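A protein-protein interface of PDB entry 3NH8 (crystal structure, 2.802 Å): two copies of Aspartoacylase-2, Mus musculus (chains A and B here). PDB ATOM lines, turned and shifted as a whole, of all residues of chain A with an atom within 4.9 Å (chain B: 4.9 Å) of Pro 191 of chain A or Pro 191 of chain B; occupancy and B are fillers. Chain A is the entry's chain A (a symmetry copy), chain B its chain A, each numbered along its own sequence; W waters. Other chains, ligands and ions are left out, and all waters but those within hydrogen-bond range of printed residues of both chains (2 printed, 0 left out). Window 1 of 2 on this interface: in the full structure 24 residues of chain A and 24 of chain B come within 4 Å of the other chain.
The side-chain amide nitrogen of Gln 190 of chain B sits close to the backbone carbonyl oxygen of Val 194 of chain B, at 3.2 Å. NE2 of Gln 190 of chain A lies close to O of Val 194 of chain A, at 3.2 Å.
Among the printed residues, merely in contact across the chains: Thr 128 of chain A with Pro 191 of chain B (3.9 Å), Thr 128 of chain A with Val 194 of chain B (3.5 Å), Pro 191 of chain A with Thr 128 of chain B (3.9 Å), Pro 191 of chain A with Pro 191 of chain B (3.9 Å), Gln 192 of chain A with Gln 192 of chain B (3.6 Å) and Val 194 of chain A with Thr 128 of chain B (3.5 Å).
Of the printed residues of chain B, Pro 191 of chain A touches Thr 128 and Pro 191. Printed residues of chain B within 4 Å of Gln 192 of chain A: Gln 192. Gly 193 of chain A touches none of the printed residues of chain B. Of the printed residues of chain A, Thr 128 of chain B touches Pro 191 and Val 194. Of chain A, only Thr 128 and Pro 191 come within 4 Å of Pro 191 of chain B. Of the printed residues of chain A, Gln 192 of chain B touches Gln 192 (3.6 Å). Printed residues of chain A within 4 Å of Val 194 of chain B: Thr 128 (3.5 Å). The nearest printed residue of chain B that does not touch Pro 191 of chain A is Gln 192 of chain B (5.0 Å). The nearest printed residue of chain A that does not touch Pro 191 of chain B is Gln 192 of chain A (5.0 Å). The nearest printed residue of chain B that does not touch Val 194 of chain A is Gln 192 of chain B (6.1 Å).
Of the 8 printed residues of chain A, 4 touch a printed residue of chain B. Hydrophobic or aromatic side chains of chain A within 4 Å of the printed part of chain B: Pro 191 and Val 194. Among the printed residues, no Asp or Glu carboxylate lies within 4 Å of a Lys or Arg side-chain nitrogen of the other chain.
Thr 128 of chain A touches Pro 191 of chain B, and with the chains exchanged Pro 191 of chain A touches Thr 128 of chain B. Thr 128 of chain A touches Val 194 of chain B, and with the chains exchanged Val 194 of chain A touches Thr 128 of chain B. Pro 191 of chain A touches its own counterpart, Pro 191 of chain B. Gln 192 of chain B touches its own counterpart, Gln 192 of chain A. Positions printed for both chains: 32, 128, 189, 190, 191, 192, 193 and 194.
Water W1 bridges the backbone carbonyl oxygen of Gln 192 of chain B and the backbone NH of Gln 192 of chain A. Water W2 lies within hydrogen-bond range of the backbone carbonyl oxygen (O) of Gln 192 of chain A and the backbone NH (N) of Gln 192 of chain B.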
ATOM      1  N   ASN A  32     -16.638 -20.701  12.266  1.00  0.00           N
ATOM      2  CA  ASN A  32     -15.511 -19.930  11.779  1.00  0.00           C
ATOM      3  C   ASN A  32     -15.074 -18.781  12.669  1.00  0.00           C
ATOM      4  O   ASN A  32     -14.220 -18.012  12.288  1.00  0.00           O
ATOM      5  CB  ASN A  32     -15.734 -19.468  10.338  1.00  0.00           C
ATOM      6  CG  ASN A  32     -17.040 -18.728  10.148  1.00  0.00           C
ATOM      7  OD1 ASN A  32     -17.803 -18.504  11.094  1.00  0.00           O
ATOM      8  ND2 ASN A  32     -17.303 -18.337   8.904  1.00  0.00           N
ATOM      9  N   THR A 128     -16.305  -9.338  12.977  1.00  0.00           N
ATOM     10  CA  THR A 128     -15.477  -8.595  12.037  1.00  0.00           C
ATOM     11  C   THR A 128     -15.686  -7.099  12.193  1.00  0.00           C
ATOM     12  O   THR A 128     -14.950  -6.321  11.612  1.00  0.00           O
ATOM     13  CB  THR A 128     -15.756  -8.957  10.546  1.00  0.00           C
ATOM     14  OG1 THR A 128     -17.061  -8.508  10.153  1.00  0.00           O
ATOM     15  CG2 THR A 128     -15.638 -10.438  10.302  1.00  0.00           C
ATOM     16  N   PRO A 189     -12.170  -6.515  16.273  1.00  0.00           N
ATOM     17  CA  PRO A 189     -12.407  -7.218  15.004  1.00  0.00           C
ATOM     18  C   PRO A 189     -11.557  -8.477  14.837  1.00  0.00           C
ATOM     19  O   PRO A 189     -10.437  -8.528  15.352  1.00  0.00           O
ATOM     20  CB  PRO A 189     -11.988  -6.178  13.946  1.00  0.00           C
ATOM     21  CG  PRO A 189     -11.512  -4.991  14.705  1.00  0.00           C
ATOM     22  CD  PRO A 189     -11.214  -5.417  16.088  1.00  0.00           C
ATOM     23  N   GLN A 190     -12.102  -9.461  14.135  1.00  0.00           N
ATOM     24  CA  GLN A 190     -11.333 -10.605  13.684  1.00  0.00           C
ATOM     25  C   GLN A 190     -11.943 -11.158  12.383  1.00  0.00           C
ATOM     26  O   GLN A 190     -13.149 -11.347  12.291  1.00  0.00           O
ATOM     27  CB  GLN A 190     -11.260 -11.682  14.785  1.00  0.00           C
ATOM     28  CG  GLN A 190     -10.096 -12.616  14.607  1.00  0.00           C
ATOM     29  CD  GLN A 190      -9.953 -13.692  15.681  1.00  0.00           C
ATOM     30  OE1 GLN A 190      -8.887 -13.823  16.287  1.00  0.00           O
ATOM     31  NE2 GLN A 190     -10.990 -14.501  15.878  1.00  0.00           N
ATOM     32  N   PRO A 191     -11.126 -11.408  11.358  1.00  0.00           N
ATOM     33  CA  PRO A 191     -11.764 -12.029  10.189  1.00  0.00           C
ATOM     34  C   PRO A 191     -12.198 -13.444  10.538  1.00  0.00           C
ATOM     35  O   PRO A 191     -11.557 -14.096  11.348  1.00  0.00           O
ATOM     36  CB  PRO A 191     -10.634 -12.089   9.148  1.00  0.00           C
ATOM     37  CG  PRO A 191      -9.559 -11.189   9.675  1.00  0.00           C
ATOM     38  CD  PRO A 191      -9.687 -11.221  11.173  1.00  0.00           C
ATOM     39  N   GLN A 192     -13.265 -13.930   9.937  1.00  0.00           N
ATOM     40  CA  GLN A 192     -13.627 -15.318  10.124  1.00  0.00           C
ATOM     41  C   GLN A 192     -12.497 -16.176   9.583  1.00  0.00           C
ATOM     42  O   GLN A 192     -11.860 -15.808   8.623  1.00  0.00           O
ATOM     43  CB  GLN A 192     -14.914 -15.613   9.372  1.00  0.00           C
ATOM     44  CG  GLN A 192     -16.065 -14.721   9.778  1.00  0.00           C
ATOM     45  CD  GLN A 192     -17.156 -14.658   8.733  1.00  0.00           C
ATOM     46  OE1 GLN A 192     -16.905 -14.297   7.576  1.00  0.00           O
ATOM     47  NE2 GLN A 192     -18.384 -14.999   9.133  1.00  0.00           N
ATOM     48  N   GLY A 193     -12.244 -17.312  10.210  1.00  0.00           N
ATOM     49  CA  GLY A 193     -11.214 -18.228   9.763  1.00  0.00           C
ATOM     50  C   GLY A 193      -9.801 -17.826  10.127  1.00  0.00           C
ATOM     51  O   GLY A 193      -8.850 -18.489   9.732  1.00  0.00           O
ATOM     52  N   VAL A 194      -9.666 -16.728  10.870  1.00  0.00           N
ATOM     53  CA  VAL A 194      -8.371 -16.203  11.288  1.00  0.00           C
ATOM     54  C   VAL A 194      -8.325 -16.188  12.794  1.00  0.00           C
ATOM     55  O   VAL A 194      -9.250 -15.735  13.445  1.00  0.00           O
ATOM     56  CB  VAL A 194      -8.136 -14.751  10.787  1.00  0.00           C
ATOM     57  CG1 VAL A 194      -6.905 -14.179  11.417  1.00  0.00           C
ATOM     58  CG2 VAL A 194      -7.983 -14.718   9.278  1.00  0.00           C
ATOM     59  N   ASN B  32     -15.686 -14.970  -1.958  1.00  0.00           N
ATOM     60  CA  ASN B  32     -15.842 -14.157  -0.769  1.00  0.00           C
ATOM     61  C   ASN B  32     -14.865 -13.003  -0.636  1.00  0.00           C
ATOM     62  O   ASN B  32     -14.843 -12.343   0.379  1.00  0.00           O
ATOM     63  CB  ASN B  32     -15.864 -15.018   0.495  1.00  0.00           C
ATOM     64  CG  ASN B  32     -14.672 -15.943   0.603  1.00  0.00           C
ATOM     65  OD1 ASN B  32     -13.772 -15.943  -0.244  1.00  0.00           O
ATOM     66  ND2 ASN B  32     -14.661 -16.745   1.665  1.00  0.00           N
ATOM     67  N   THR B 128      -6.753 -11.228   4.035  1.00  0.00           N
ATOM     68  CA  THR B 128      -6.932 -10.911   5.446  1.00  0.00           C
ATOM     69  C   THR B 128      -5.602 -10.580   6.101  1.00  0.00           C
ATOM     70  O   THR B 128      -5.580 -10.124   7.231  1.00  0.00           O
ATOM     71  CB  THR B 128      -7.584 -12.069   6.263  1.00  0.00           C
ATOM     72  OG1 THR B 128      -6.689 -13.186   6.359  1.00  0.00           O
ATOM     73  CG2 THR B 128      -8.885 -12.516   5.651  1.00  0.00           C
ATOM     74  N   PRO B 189      -5.568  -5.378   4.590  1.00  0.00           N
ATOM     75  CA  PRO B 189      -6.432  -6.470   5.062  1.00  0.00           C
ATOM     76  C   PRO B 189      -7.915  -6.243   4.771  1.00  0.00           C
ATOM     77  O   PRO B 189      -8.360  -5.092   4.744  1.00  0.00           O
ATOM     78  CB  PRO B 189      -6.206  -6.458   6.588  1.00  0.00           C
ATOM     79  CG  PRO B 189      -5.266  -5.336   6.853  1.00  0.00           C
ATOM     80  CD  PRO B 189      -5.275  -4.439   5.679  1.00  0.00           C
ATOM     81  N   GLN B 190      -8.641  -7.330   4.554  1.00  0.00           N
ATOM     82  CA  GLN B 190     -10.091  -7.295   4.512  1.00  0.00           C
ATOM     83  C   GLN B 190     -10.653  -8.656   4.964  1.00  0.00           C
ATOM     84  O   GLN B 190     -10.204  -9.699   4.508  1.00  0.00           O
ATOM     85  CB  GLN B 190     -10.587  -6.909   3.105  1.00  0.00           C
ATOM     86  CG  GLN B 190     -11.985  -6.355   3.114  1.00  0.00           C
ATOM     87  CD  GLN B 190     -12.526  -5.930   1.751  1.00  0.00           C
ATOM     88  OE1 GLN B 190     -12.974  -4.792   1.592  1.00  0.00           O
ATOM     89  NE2 GLN B 190     -12.548  -6.847   0.789  1.00  0.00           N
ATOM     90  N   PRO B 191     -11.629  -8.665   5.874  1.00  0.00           N
ATOM     91  CA  PRO B 191     -12.186  -9.990   6.179  1.00  0.00           C
ATOM     92  C   PRO B 191     -12.942 -10.515   4.968  1.00  0.00           C
ATOM     93  O   PRO B 191     -13.504  -9.735   4.215  1.00  0.00           O
ATOM     94  CB  PRO B 191     -13.183  -9.712   7.317  1.00  0.00           C
ATOM     95  CG  PRO B 191     -12.859  -8.333   7.802  1.00  0.00           C
ATOM     96  CD  PRO B 191     -12.299  -7.596   6.617  1.00  0.00           C
ATOM     97  N   GLN B 192     -12.973 -11.818   4.776  1.00  0.00           N
ATOM     98  CA  GLN B 192     -13.801 -12.371   3.727  1.00  0.00           C
ATOM     99  C   GLN B 192     -15.247 -12.028   4.039  1.00  0.00           C
ATOM    100  O   GLN B 192     -15.626 -11.973   5.187  1.00  0.00           O
ATOM    101  CB  GLN B 192     -13.620 -13.879   3.678  1.00  0.00           C
ATOM    102  CG  GLN B 192     -12.184 -14.306   3.480  1.00  0.00           C
ATOM    103  CD  GLN B 192     -11.926 -15.729   3.920  1.00  0.00           C
ATOM    104  OE1 GLN B 192     -12.177 -16.088   5.078  1.00  0.00           O
ATOM    105  NE2 GLN B 192     -11.413 -16.554   3.003  1.00  0.00           N
ATOM    106  N   GLY B 193     -16.047 -11.785   3.016  1.00  0.00           N
ATOM    107  CA  GLY B 193     -17.454 -11.483   3.190  1.00  0.00           C
ATOM    108  C   GLY B 193     -17.751 -10.066   3.633  1.00  0.00           C
ATOM    109  O   GLY B 193     -18.901  -9.728   3.885  1.00  0.00           O
ATOM    110  N   VAL B 194     -16.709  -9.243   3.743  1.00  0.00           N
ATOM    111  CA  VAL B 194     -16.829  -7.856   4.174  1.00  0.00           C
ATOM    112  C   VAL B 194     -16.322  -6.966   3.070  1.00  0.00           C
ATOM    113  O   VAL B 194     -15.260  -7.198   2.518  1.00  0.00           O
ATOM    114  CB  VAL B 194     -15.994  -7.561   5.450  1.00  0.00           C
ATOM    115  CG1 VAL B 194     -15.972  -6.091   5.727  1.00  0.00           C
ATOM    116  CG2 VAL B 194     -16.570  -8.285   6.653  1.00  0.00           C
HETATM  117  O   HOH W   1     -14.450 -12.501   7.623  1.00  0.00           O
HETATM  118  O   HOH W   2     -12.042 -13.660   6.907  1.00  0.00           O
